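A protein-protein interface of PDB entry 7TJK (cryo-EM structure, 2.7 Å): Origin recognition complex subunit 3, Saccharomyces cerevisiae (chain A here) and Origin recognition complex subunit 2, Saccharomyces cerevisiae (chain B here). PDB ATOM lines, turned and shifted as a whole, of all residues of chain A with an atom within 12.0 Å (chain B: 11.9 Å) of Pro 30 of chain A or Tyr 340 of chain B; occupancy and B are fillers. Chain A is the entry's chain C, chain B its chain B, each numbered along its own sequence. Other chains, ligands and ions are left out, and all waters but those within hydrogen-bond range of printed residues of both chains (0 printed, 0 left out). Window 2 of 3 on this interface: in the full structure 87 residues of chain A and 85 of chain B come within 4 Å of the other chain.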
ATOM      1  N   TYR A  26     -33.179   2.449  29.712  1.00  0.00           N
ATOM      2  CA  TYR A  26     -32.706   1.712  28.547  1.00  0.00           C
ATOM      3  C   TYR A  26     -31.186   1.672  28.568  1.00  0.00           C
ATOM      4  O   TYR A  26     -30.544   2.706  28.323  1.00  0.00           O
ATOM      5  CB  TYR A  26     -33.212   2.356  27.257  1.00  0.00           C
ATOM      6  CG  TYR A  26     -34.704   2.208  27.054  1.00  0.00           C
ATOM      7  CD1 TYR A  26     -35.592   3.147  27.567  1.00  0.00           C
ATOM      8  CD2 TYR A  26     -35.224   1.128  26.350  1.00  0.00           C
ATOM      9  CE1 TYR A  26     -36.954   3.014  27.384  1.00  0.00           C
ATOM     10  CE2 TYR A  26     -36.586   0.987  26.162  1.00  0.00           C
ATOM     11  CZ  TYR A  26     -37.445   1.933  26.681  1.00  0.00           C
ATOM     12  OH  TYR A  26     -38.801   1.798  26.497  1.00  0.00           O
ATOM     13  N   PRO A  27     -30.578   0.540  28.922  1.00  0.00           N
ATOM     14  CA  PRO A  27     -29.120   0.412  28.885  1.00  0.00           C
ATOM     15  C   PRO A  27     -28.541   0.626  27.491  1.00  0.00           C
ATOM     16  O   PRO A  27     -29.172   0.358  26.468  1.00  0.00           O
ATOM     17  CB  PRO A  27     -28.922  -1.042  29.314  1.00  0.00           C
ATOM     18  CG  PRO A  27     -30.070  -1.311  30.270  1.00  0.00           C
ATOM     19  CD  PRO A  27     -31.080  -0.184  30.102  1.00  0.00           C
ATOM     20  N   SER A  28     -27.312   1.126  27.474  1.00  0.00           N
ATOM     21  CA  SER A  28     -26.562   1.289  26.242  1.00  0.00           C
ATOM     22  C   SER A  28     -25.851  -0.012  25.883  1.00  0.00           C
ATOM     23  O   SER A  28     -25.673  -0.904  26.715  1.00  0.00           O
ATOM     24  CB  SER A  28     -25.549   2.426  26.373  1.00  0.00           C
ATOM     25  OG  SER A  28     -26.198   3.660  26.617  1.00  0.00           O
ATOM     26  N   LEU A  29     -25.444  -0.108  24.619  1.00  0.00           N
ATOM     27  CA  LEU A  29     -24.737  -1.276  24.121  1.00  0.00           C
ATOM     28  C   LEU A  29     -23.639  -0.818  23.170  1.00  0.00           C
ATOM     29  O   LEU A  29     -23.861   0.091  22.356  1.00  0.00           O
ATOM     30  CB  LEU A  29     -25.682  -2.276  23.423  1.00  0.00           C
ATOM     31  CG  LEU A  29     -26.339  -2.047  22.054  1.00  0.00           C
ATOM     32  CD1 LEU A  29     -26.877  -3.361  21.515  1.00  0.00           C
ATOM     33  CD2 LEU A  29     -27.461  -1.018  22.110  1.00  0.00           C
ATOM     34  N   PRO A  30     -22.433  -1.400  23.271  1.00  0.00           N
ATOM     35  CA  PRO A  30     -21.303  -0.990  22.428  1.00  0.00           C
ATOM     36  C   PRO A  30     -21.342  -1.587  21.023  1.00  0.00           C
ATOM     37  O   PRO A  30     -22.379  -1.528  20.363  1.00  0.00           O
ATOM     38  CB  PRO A  30     -20.092  -1.514  23.200  1.00  0.00           C
ATOM     39  CG  PRO A  30     -20.609  -2.715  23.908  1.00  0.00           C
ATOM     40  CD  PRO A  30     -22.027  -2.387  24.289  1.00  0.00           C
ATOM     41  N   HIS A  38     -21.659 -15.408  23.039  1.00  0.00           N
ATOM     42  CA  HIS A  38     -22.645 -14.791  23.915  1.00  0.00           C
ATOM     43  C   HIS A  38     -23.456 -15.838  24.669  1.00  0.00           C
ATOM     44  O   HIS A  38     -24.683 -15.857  24.589  1.00  0.00           O
ATOM     45  CB  HIS A  38     -23.586 -13.891  23.113  1.00  0.00           C
ATOM     46  CG  HIS A  38     -22.912 -12.709  22.492  1.00  0.00           C
ATOM     47  ND1 HIS A  38     -23.180 -12.291  21.206  1.00  0.00           N
ATOM     48  CD2 HIS A  38     -21.980 -11.855  22.978  1.00  0.00           C
ATOM     49  CE1 HIS A  38     -22.443 -11.232  20.926  1.00  0.00           C
ATOM     50  NE2 HIS A  38     -21.706 -10.945  21.985  1.00  0.00           N
ATOM     51  N   ILE A  39     -22.772 -16.711  25.402  1.00  0.00           N
ATOM     52  CA  ILE A  39     -23.448 -17.742  26.186  1.00  0.00           C
ATOM     53  C   ILE A  39     -22.987 -17.643  27.637  1.00  0.00           C
ATOM     54  O   ILE A  39     -21.846 -17.234  27.897  1.00  0.00           O
ATOM     55  CB  ILE A  39     -23.198 -19.145  25.602  1.00  0.00           C
ATOM     56  CG1 ILE A  39     -21.705 -19.424  25.453  1.00  0.00           C
ATOM     57  CG2 ILE A  39     -23.919 -19.315  24.270  1.00  0.00           C
ATOM     58  CD1 ILE A  39     -21.406 -20.846  25.076  1.00  0.00           C
ATOM     59  N   PRO A  40     -23.836 -17.978  28.610  1.00  0.00           N
ATOM     60  CA  PRO A  40     -23.440 -17.885  30.020  1.00  0.00           C
ATOM     61  C   PRO A  40     -22.496 -18.975  30.504  1.00  0.00           C
ATOM     62  O   PRO A  40     -22.095 -18.933  31.669  1.00  0.00           O
ATOM     63  CB  PRO A  40     -24.786 -17.982  30.757  1.00  0.00           C
ATOM     64  CG  PRO A  40     -25.699 -18.644  29.809  1.00  0.00           C
ATOM     65  CD  PRO A  40     -25.289 -18.164  28.465  1.00  0.00           C
ATOM     66  N   GLU A  55     -18.897 -24.407  23.716  1.00  0.00           N
ATOM     67  CA  GLU A  55     -20.008 -24.404  22.764  1.00  0.00           C
ATOM     68  C   GLU A  55     -20.660 -25.779  22.642  1.00  0.00           C
ATOM     69  O   GLU A  55     -21.896 -25.876  22.576  1.00  0.00           O
ATOM     70  CB  GLU A  55     -19.525 -23.933  21.393  1.00  0.00           C
ATOM     71  CG  GLU A  55     -19.071 -22.481  21.334  1.00  0.00           C
ATOM     72  CD  GLU A  55     -20.203 -21.494  21.542  1.00  0.00           C
ATOM     73  OE1 GLU A  55     -21.348 -21.800  21.146  1.00  0.00           O
ATOM     74  OE2 GLU A  55     -19.945 -20.404  22.096  1.00  0.00           O
ATOM     75  N   TRP A  58     -22.750 -26.378  25.743  1.00  0.00           N
ATOM     76  CA  TRP A  58     -23.992 -25.617  25.590  1.00  0.00           C
ATOM     77  C   TRP A  58     -24.998 -26.357  24.709  1.00  0.00           C
ATOM     78  O   TRP A  58     -26.174 -26.512  25.075  1.00  0.00           O
ATOM     79  CB  TRP A  58     -23.654 -24.247  24.999  1.00  0.00           C
ATOM     80  CG  TRP A  58     -24.774 -23.261  24.844  1.00  0.00           C
ATOM     81  CD1 TRP A  58     -25.263 -22.762  23.675  1.00  0.00           C
ATOM     82  CD2 TRP A  58     -25.485 -22.591  25.893  1.00  0.00           C
ATOM     83  NE1 TRP A  58     -26.260 -21.851  23.927  1.00  0.00           N
ATOM     84  CE2 TRP A  58     -26.415 -21.727  25.281  1.00  0.00           C
ATOM     85  CE3 TRP A  58     -25.443 -22.655  27.290  1.00  0.00           C
ATOM     86  CZ2 TRP A  58     -27.283 -20.922  26.016  1.00  0.00           C
ATOM     87  CZ3 TRP A  58     -26.312 -21.865  28.016  1.00  0.00           C
ATOM     88  CH2 TRP A  58     -27.223 -21.015  27.379  1.00  0.00           C
ATOM     89  N   TRP B 305     -27.325 -15.414  34.835  1.00  0.00           N
ATOM     90  CA  TRP B 305     -27.885 -15.270  33.493  1.00  0.00           C
ATOM     91  C   TRP B 305     -28.364 -16.628  32.975  1.00  0.00           C
ATOM     92  O   TRP B 305     -29.433 -16.725  32.356  1.00  0.00           O
ATOM     93  CB  TRP B 305     -26.819 -14.652  32.573  1.00  0.00           C
ATOM     94  CG  TRP B 305     -27.075 -14.595  31.068  1.00  0.00           C
ATOM     95  CD1 TRP B 305     -28.275 -14.661  30.419  1.00  0.00           C
ATOM     96  CD2 TRP B 305     -26.080 -14.525  30.041  1.00  0.00           C
ATOM     97  NE1 TRP B 305     -28.092 -14.601  29.063  1.00  0.00           N
ATOM     98  CE2 TRP B 305     -26.751 -14.522  28.804  1.00  0.00           C
ATOM     99  CE3 TRP B 305     -24.684 -14.448  30.049  1.00  0.00           C
ATOM    100  CZ2 TRP B 305     -26.076 -14.447  27.589  1.00  0.00           C
ATOM    101  CZ3 TRP B 305     -24.019 -14.384  28.842  1.00  0.00           C
ATOM    102  CH2 TRP B 305     -24.713 -14.375  27.631  1.00  0.00           C
ATOM    103  N   THR B 309     -32.216 -17.573  31.821  1.00  0.00           N
ATOM    104  CA  THR B 309     -32.630 -18.057  30.504  1.00  0.00           C
ATOM    105  C   THR B 309     -33.329 -19.408  30.550  1.00  0.00           C
ATOM    106  O   THR B 309     -33.906 -19.817  29.538  1.00  0.00           O
ATOM    107  CB  THR B 309     -31.438 -18.155  29.551  1.00  0.00           C
ATOM    108  OG1 THR B 309     -30.462 -19.057  30.088  1.00  0.00           O
ATOM    109  CG2 THR B 309     -30.823 -16.794  29.320  1.00  0.00           C
ATOM    110  N   ALA B 330     -28.389  -6.138  36.537  1.00  0.00           N
ATOM    111  CA  ALA B 330     -29.429  -6.135  35.513  1.00  0.00           C
ATOM    112  C   ALA B 330     -29.116  -5.179  34.369  1.00  0.00           C
ATOM    113  O   ALA B 330     -29.317  -5.523  33.199  1.00  0.00           O
ATOM    114  CB  ALA B 330     -30.773  -5.782  36.140  1.00  0.00           C
ATOM    115  N   ILE B 331     -28.626  -3.984  34.682  1.00  0.00           N
ATOM    116  CA  ILE B 331     -28.437  -2.949  33.671  1.00  0.00           C
ATOM    117  C   ILE B 331     -27.092  -3.084  32.968  1.00  0.00           C
ATOM    118  O   ILE B 331     -27.034  -3.150  31.738  1.00  0.00           O
ATOM    119  CB  ILE B 331     -28.600  -1.562  34.324  1.00  0.00           C
ATOM    120  CG1 ILE B 331     -30.023  -1.391  34.863  1.00  0.00           C
ATOM    121  CG2 ILE B 331     -28.232  -0.455  33.354  1.00  0.00           C
ATOM    122  CD1 ILE B 331     -30.200  -0.176  35.741  1.00  0.00           C
ATOM    123  N   ASP B 332     -25.997  -3.136  33.725  1.00  0.00           N
ATOM    124  CA  ASP B 332     -24.664  -3.148  33.140  1.00  0.00           C
ATOM    125  C   ASP B 332     -24.269  -4.491  32.539  1.00  0.00           C
ATOM    126  O   ASP B 332     -23.520  -4.512  31.556  1.00  0.00           O
ATOM    127  CB  ASP B 332     -23.624  -2.745  34.189  1.00  0.00           C
ATOM    128  CG  ASP B 332     -23.874  -1.361  34.757  1.00  0.00           C
ATOM    129  OD1 ASP B 332     -24.433  -0.509  34.035  1.00  0.00           O
ATOM    130  OD2 ASP B 332     -23.510  -1.124  35.928  1.00  0.00           O
ATOM    131  N   TYR B 333     -24.748  -5.603  33.089  1.00  0.00           N
ATOM    132  CA  TYR B 333     -24.316  -6.922  32.643  1.00  0.00           C
ATOM    133  C   TYR B 333     -25.397  -7.673  31.883  1.00  0.00           C
ATOM    134  O   TYR B 333     -25.159  -8.116  30.755  1.00  0.00           O
ATOM    135  CB  TYR B 333     -23.849  -7.758  33.853  1.00  0.00           C
ATOM    136  CG  TYR B 333     -23.330  -9.145  33.511  1.00  0.00           C
ATOM    137  CD1 TYR B 333     -22.007  -9.334  33.129  1.00  0.00           C
ATOM    138  CD2 TYR B 333     -24.156 -10.267  33.590  1.00  0.00           C
ATOM    139  CE1 TYR B 333     -21.526 -10.596  32.821  1.00  0.00           C
ATOM    140  CE2 TYR B 333     -23.686 -11.526  33.273  1.00  0.00           C
ATOM    141  CZ  TYR B 333     -22.370 -11.684  32.894  1.00  0.00           C
ATOM    142  OH  TYR B 333     -21.897 -12.937  32.588  1.00  0.00           O
ATOM    143  N   LEU B 334     -26.576  -7.844  32.481  1.00  0.00           N
ATOM    144  CA  LEU B 334     -27.561  -8.788  31.964  1.00  0.00           C
ATOM    145  C   LEU B 334     -28.260  -8.273  30.711  1.00  0.00           C
ATOM    146  O   LEU B 334     -28.445  -9.025  29.749  1.00  0.00           O
ATOM    147  CB  LEU B 334     -28.584  -9.108  33.050  1.00  0.00           C
ATOM    148  CG  LEU B 334     -29.685 -10.093  32.688  1.00  0.00           C
ATOM    149  CD1 LEU B 334     -29.216 -11.516  32.916  1.00  0.00           C
ATOM    150  CD2 LEU B 334     -30.912  -9.787  33.509  1.00  0.00           C
ATOM    151  N   SER B 335     -28.661  -6.997  30.715  1.00  0.00           N
ATOM    152  CA  SER B 335     -29.377  -6.416  29.576  1.00  0.00           C
ATOM    153  C   SER B 335     -28.603  -6.424  28.253  1.00  0.00           C
ATOM    154  O   SER B 335     -29.152  -6.946  27.263  1.00  0.00           O
ATOM    155  CB  SER B 335     -29.852  -5.005  29.941  1.00  0.00           C
ATOM    156  OG  SER B 335     -30.336  -4.317  28.802  1.00  0.00           O
ATOM    157  N   PRO B 336     -27.356  -5.916  28.142  1.00  0.00           N
ATOM    158  CA  PRO B 336     -26.723  -5.951  26.813  1.00  0.00           C
ATOM    159  C   PRO B 336     -26.249  -7.331  26.399  1.00  0.00           C
ATOM    160  O   PRO B 336     -26.175  -7.604  25.199  1.00  0.00           O
ATOM    161  CB  PRO B 336     -25.559  -4.955  26.933  1.00  0.00           C
ATOM    162  CG  PRO B 336     -25.465  -4.578  28.361  1.00  0.00           C
ATOM    163  CD  PRO B 336     -26.373  -5.444  29.142  1.00  0.00           C
ATOM    164  N   LYS B 337     -25.972  -8.230  27.344  1.00  0.00           N
ATOM    165  CA  LYS B 337     -25.569  -9.577  26.961  1.00  0.00           C
ATOM    166  C   LYS B 337     -26.761 -10.436  26.543  1.00  0.00           C
ATOM    167  O   LYS B 337     -26.616 -11.292  25.662  1.00  0.00           O
ATOM    168  CB  LYS B 337     -24.774 -10.214  28.101  1.00  0.00           C
ATOM    169  CG  LYS B 337     -23.425  -9.524  28.281  1.00  0.00           C
ATOM    170  CD  LYS B 337     -22.616 -10.057  29.442  1.00  0.00           C
ATOM    171  CE  LYS B 337     -22.090 -11.446  29.172  1.00  0.00           C
ATOM    172  NZ  LYS B 337     -21.065 -11.477  28.096  1.00  0.00           N
ATOM    173  N   ILE B 338     -27.942 -10.212  27.135  1.00  0.00           N
ATOM    174  CA  ILE B 338     -29.162 -10.824  26.611  1.00  0.00           C
ATOM    175  C   ILE B 338     -29.503 -10.242  25.242  1.00  0.00           C
ATOM    176  O   ILE B 338     -29.906 -10.976  24.328  1.00  0.00           O
ATOM    177  CB  ILE B 338     -30.324 -10.678  27.621  1.00  0.00           C
ATOM    178  CG1 ILE B 338     -30.125 -11.631  28.804  1.00  0.00           C
ATOM    179  CG2 ILE B 338     -31.702 -10.903  26.972  1.00  0.00           C
ATOM    180  CD1 ILE B 338     -31.309 -11.709  29.750  1.00  0.00           C
ATOM    181  N   ALA B 339     -29.309  -8.928  25.063  1.00  0.00           N
ATOM    182  CA  ALA B 339     -29.548  -8.312  23.760  1.00  0.00           C
ATOM    183  C   ALA B 339     -28.588  -8.832  22.692  1.00  0.00           C
ATOM    184  O   ALA B 339     -28.991  -9.020  21.538  1.00  0.00           O
ATOM    185  CB  ALA B 339     -29.443  -6.791  23.874  1.00  0.00           C
ATOM    186  N   TYR B 340     -27.332  -9.084  23.056  1.00  0.00           N
ATOM    187  CA  TYR B 340     -26.367  -9.629  22.111  1.00  0.00           C
ATOM    188  C   TYR B 340     -26.592 -11.112  21.842  1.00  0.00           C
ATOM    189  O   TYR B 340     -26.313 -11.581  20.733  1.00  0.00           O
ATOM    190  CB  TYR B 340     -24.947  -9.403  22.628  1.00  0.00           C
ATOM    191  CG  TYR B 340     -24.421  -8.014  22.358  1.00  0.00           C
ATOM    192  CD1 TYR B 340     -24.884  -7.277  21.274  1.00  0.00           C
ATOM    193  CD2 TYR B 340     -23.470  -7.438  23.189  1.00  0.00           C
ATOM    194  CE1 TYR B 340     -24.409  -6.004  21.022  1.00  0.00           C
ATOM    195  CE2 TYR B 340     -22.990  -6.165  22.947  1.00  0.00           C
ATOM    196  CZ  TYR B 340     -23.463  -5.455  21.862  1.00  0.00           C
ATOM    197  OH  TYR B 340     -22.989  -4.190  21.616  1.00  0.00           O
ATOM    198  N   SER B 341     -27.092 -11.860  22.827  1.00  0.00           N
ATOM    199  CA  SER B 341     -27.284 -13.294  22.643  1.00  0.00           C
ATOM    200  C   SER B 341     -28.490 -13.618  21.771  1.00  0.00           C
ATOM    201  O   SER B 341     -28.627 -14.762  21.328  1.00  0.00           O
ATOM    202  CB  SER B 341     -27.428 -13.982  24.001  1.00  0.00           C
ATOM    203  OG  SER B 341     -28.574 -13.514  24.689  1.00  0.00           O
ATOM    204  N   GLN B 342     -29.366 -12.646  21.520  1.00  0.00           N
ATOM    205  CA  GLN B 342     -30.561 -12.854  20.715  1.00  0.00           C
ATOM    206  C   GLN B 342     -30.527 -12.081  19.404  1.00  0.00           C
ATOM    207  O   GLN B 342     -31.575 -11.903  18.774  1.00  0.00           O
ATOM    208  CB  GLN B 342     -31.805 -12.478  21.522  1.00  0.00           C
ATOM    209  CG  GLN B 342     -31.900 -13.202  22.854  1.00  0.00           C
ATOM    210  CD  GLN B 342     -33.037 -12.698  23.717  1.00  0.00           C
ATOM    211  OE1 GLN B 342     -33.679 -13.470  24.429  1.00  0.00           O
ATOM    212  NE2 GLN B 342     -33.289 -11.396  23.664  1.00  0.00           N
ATOM    213  N   LEU B 343     -29.356 -11.620  18.978  1.00  0.00           N
ATOM    214  CA  LEU B 343     -29.230 -10.900  17.716  1.00  0.00           C
ATOM    215  C   LEU B 343     -29.137 -11.867  16.542  1.00  0.00           C
ATOM    216  O   LEU B 343     -30.150 -12.378  16.064  1.00  0.00           O
ATOM    217  CB  LEU B 343     -28.005  -9.984  17.739  1.00  0.00           C
ATOM    218  CG  LEU B 343     -28.229  -8.564  18.266  1.00  0.00           C
ATOM    219  CD1 LEU B 343     -26.933  -7.771  18.238  1.00  0.00           C
ATOM    220  CD2 LEU B 343     -29.314  -7.857  17.467  1.00  0.00           C
ATOM    221  N   SER B 357     -31.035  -2.037  23.579  1.00  0.00           N
ATOM    222  CA  SER B 357     -30.956  -3.170  24.493  1.00  0.00           C
ATOM    223  C   SER B 357     -32.317  -3.481  25.106  1.00  0.00           C
ATOM    224  O   SER B 357     -33.312  -2.825  24.797  1.00  0.00           O
ATOM    225  CB  SER B 357     -29.937  -2.896  25.601  1.00  0.00           C
ATOM    226  OG  SER B 357     -30.488  -2.044  26.589  1.00  0.00           O
ATOM    227  N   ILE B 358     -32.349  -4.481  25.973  1.00  0.00           N
ATOM    228  CA  ILE B 358     -33.569  -4.913  26.651  1.00  0.00           C
ATOM    229  C   ILE B 358     -33.927  -3.864  27.699  1.00  0.00           C
ATOM    230  O   ILE B 358     -33.049  -3.465  28.477  1.00  0.00           O
ATOM    231  CB  ILE B 358     -33.394  -6.297  27.303  1.00  0.00           C
ATOM    232  CG1 ILE B 358     -32.614  -7.239  26.379  1.00  0.00           C
ATOM    233  CG2 ILE B 358     -34.747  -6.902  27.658  1.00  0.00           C
ATOM    234  CD1 ILE B 358     -33.331  -7.586  25.091  1.00  0.00           C
ATOM    235  N   PRO B 359     -35.169  -3.377  27.735  1.00  0.00           N
ATOM    236  CA  PRO B 359     -35.547  -2.396  28.760  1.00  0.00           C
ATOM    237  C   PRO B 359     -35.592  -3.011  30.151  1.00  0.00           C
ATOM    238  O   PRO B 359     -35.884  -4.196  30.322  1.00  0.00           O
ATOM    239  CB  PRO B 359     -36.936  -1.932  28.312  1.00  0.00           C
ATOM    240  CG  PRO B 359     -37.460  -3.065  27.499  1.00  0.00           C
ATOM    241  CD  PRO B 359     -36.275  -3.645  26.798  1.00  0.00           C
ATOM    242  N   LEU B 416     -39.244 -17.793  22.566  1.00  0.00           N
ATOM    243  CA  LEU B 416     -38.813 -17.599  23.953  1.00  0.00           C
ATOM    244  C   LEU B 416     -37.600 -16.671  23.980  1.00  0.00           C
ATOM    245  O   LEU B 416     -36.471 -17.069  24.277  1.00  0.00           O
ATOM    246  CB  LEU B 416     -38.510 -18.937  24.619  1.00  0.00           C
ATOM    247  CG  LEU B 416     -39.629 -19.795  25.232  1.00  0.00           C
ATOM    248  CD1 LEU B 416     -40.637 -20.322  24.214  1.00  0.00           C
ATOM    249  CD2 LEU B 416     -39.023 -20.953  26.008  1.00  0.00           C
ATOM    250  N   ASP B 417     -37.850 -15.404  23.662  1.00  0.00           N
ATOM    251  CA  ASP B 417     -36.850 -14.346  23.707  1.00  0.00           C
ATOM    252  C   ASP B 417     -37.232 -13.374  24.811  1.00  0.00           C
ATOM    253  O   ASP B 417     -38.383 -12.933  24.879  1.00  0.00           O
ATOM    254  CB  ASP B 417     -36.748 -13.592  22.372  1.00  0.00           C
ATOM    255  CG  ASP B 417     -36.497 -14.507  21.178  1.00  0.00           C
ATOM    256  OD1 ASP B 417     -36.353 -15.733  21.353  1.00  0.00           O
ATOM    257  OD2 ASP B 417     -36.443 -13.986  20.045  1.00  0.00           O
ATOM    258  N   ILE B 418     -36.301 -13.013  25.665  1.00  0.00           N
ATOM    259  CA  ILE B 418     -36.547 -12.063  26.766  1.00  0.00           C
ATOM    260  C   ILE B 418     -36.761 -10.599  26.298  1.00  0.00           C
ATOM    261  O   ILE B 418     -35.807  -9.881  26.198  1.00  0.00           O
ATOM    262  CB  ILE B 418     -35.437 -12.234  27.819  1.00  0.00           C
ATOM    263  CG1 ILE B 418     -35.639 -13.492  28.662  1.00  0.00           C
ATOM    264  CG2 ILE B 418     -35.328 -11.003  28.706  1.00  0.00           C
ATOM    265  CD1 ILE B 418     -34.577 -13.680  29.713  1.00  0.00           C
ATOM    266  N   LYS B 419     -38.006 -10.148  26.255  1.00  0.00           N
ATOM    267  CA  LYS B 419     -38.411  -8.774  25.895  1.00  0.00           C
ATOM    268  C   LYS B 419     -38.275  -7.742  27.006  1.00  0.00           C
ATOM    269  O   LYS B 419     -38.286  -6.611  26.658  1.00  0.00           O
ATOM    270  CB  LYS B 419     -39.874  -8.844  25.488  1.00  0.00           C
ATOM    271  CG  LYS B 419     -40.161  -9.530  24.168  1.00  0.00           C
ATOM    272  CD  LYS B 419     -41.168 -10.648  24.278  1.00  0.00           C
ATOM    273  CE  LYS B 419     -41.126 -11.545  23.063  1.00  0.00           C
ATOM    274  NZ  LYS B 419     -39.926 -11.259  22.249  1.00  0.00           N
ATOM    275  N   ILE B 421     -36.669  -6.807  31.234  1.00  0.00           N
ATOM    276  CA  ILE B 421     -35.980  -7.153  32.470  1.00  0.00           C
ATOM    277  C   ILE B 421     -36.698  -6.441  33.604  1.00  0.00           C
ATOM    278  O   ILE B 421     -36.677  -5.207  33.682  1.00  0.00           O
ATOM    279  CB  ILE B 421     -34.499  -6.754  32.425  1.00  0.00           C
ATOM    280  CG1 ILE B 421     -33.793  -7.444  31.258  1.00  0.00           C
ATOM    281  CG2 ILE B 421     -33.821  -7.100  33.739  1.00  0.00           C
ATOM    282  CD1 ILE B 421     -33.807  -8.937  31.332  1.00  0.00           C
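ND1 of His 38 of chain A lies within hydrogen-bond range of O of Tyr 340 of chain B, at 3.2 Å. The side-chain hydroxyl (OH) of Tyr 340 of chain B is in hydrogen-bond range of the backbone carbonyl oxygen (O) of Pro 30 of chain A, at 3.0 Å. The backbone carbonyl oxygen (O) of Pro 27 of chain A is in hydrogen-bond range of the side-chain hydroxyl (OG) of Ser 357 of chain B (2.7 Å).
The backbone carbonyl oxygen (O) of Trp 305 of chain B sits close to the side-chain hydroxyl (OG1) of Thr 309 of chain B. OG of Ser 335 of chain B sits at hydrogen-bond distance from O of Ile 358 of chain B (2.9 Å). The backbone carbonyl oxygen (O) of Ile 338 of chain B sits at hydrogen-bond distance from the side-chain hydroxyl (OG) of Ser 341 of chain B (2.9 Å). O of Lys 337 of chain B lies within hydrogen-bond range of OG of Ser 341 of chain B (3.1 Å). O of Pro 359 of chain B sits at hydrogen-bond distance from N of Ile 421 of chain B (2.9 Å). OG of Ser 335 of chain B sits at hydrogen-bond distance from OG of Ser 357 of chain B, at 3.2 Å.
Among the printed residues, pairs that only touch across the chains: Tyr 26 of chain A with Pro 359 of chain B, Pro 27 of chain A with Ile 331 of chain B, Pro 27 of chain A with Ser 335 of chain B, Leu 29 of chain A with Tyr 340 of chain B, Leu 29 of chain A with Ser 357 of chain B, His 38 of chain A with Trp 305 of chain B, His 38 of chain A with Ser 341 of chain B, Ile 39 of chain A with Trp 305 of chain B and Pro 40 of chain A with Trp 305 of chain B.
Tyr 340 of chain B touches just these residues of chain A: Leu 29 (3.6 Å), Pro 30 (3.0 Å) and His 38 (3.2 Å). No residue of chain B comes within 4 Å of Ser 28 of chain A. No residue of chain A comes within 4 Å of Lys 337 of chain B. No residue of chain A comes within 4 Å of Ala 339 of chain B. No residue of chain A comes within 4 Å of Gln 342 of chain B. No residue of chain A comes within 4 Å of Leu 343 of chain B. Printed residues of chain B within 4 Å of Leu 29 of chain A: Tyr 340 (3.6 Å) and Ser 357 (3.996 Å). Printed residues of chain A within 4 Å of Trp 305 of chain B: His 38, Ile 39 and Pro 40. Printed residues of chain B within 4 Å of Pro 40 of chain A: Trp 305 (3.6 Å). Printed residues of chain A within 4 Å of Ile 331 of chain B: Pro 27 (3.7 Å). Asp 332 of chain B touches none of the printed residues of chain A. The nearest printed residue of chain A that does not touch Pro 359 of chain B is Pro 27 of chain A (5.2 Å).
Hydrophobic or aromatic side chains of chain A that line the printed part of chain B: Tyr 26, Pro 27, Leu 29, Pro 30, His 38 and Pro 40. Along chain A the printed residues that touch a printed residue of chain B span positions 26 to 40. Of the 24 printed residues of chain B, 7 touch a printed residue of chain A. Printed residues of chain B that touch a printed residue of chain A: Trp 305, Ile 331, Ser 335, Tyr 340, Ser 341, Ser 357 and Pro 359. Hydrophobic or aromatic side chains of chain B that line the printed part of chain A: Trp 305, Ile 331, Tyr 340 and Pro 359. Among the printed residues, 12 pairs touch across the chains. Among the printed residues, no Asp or Glu carboxylate lies within 4 Å of a Lys or Arg side-chain nitrogen of the other chain.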
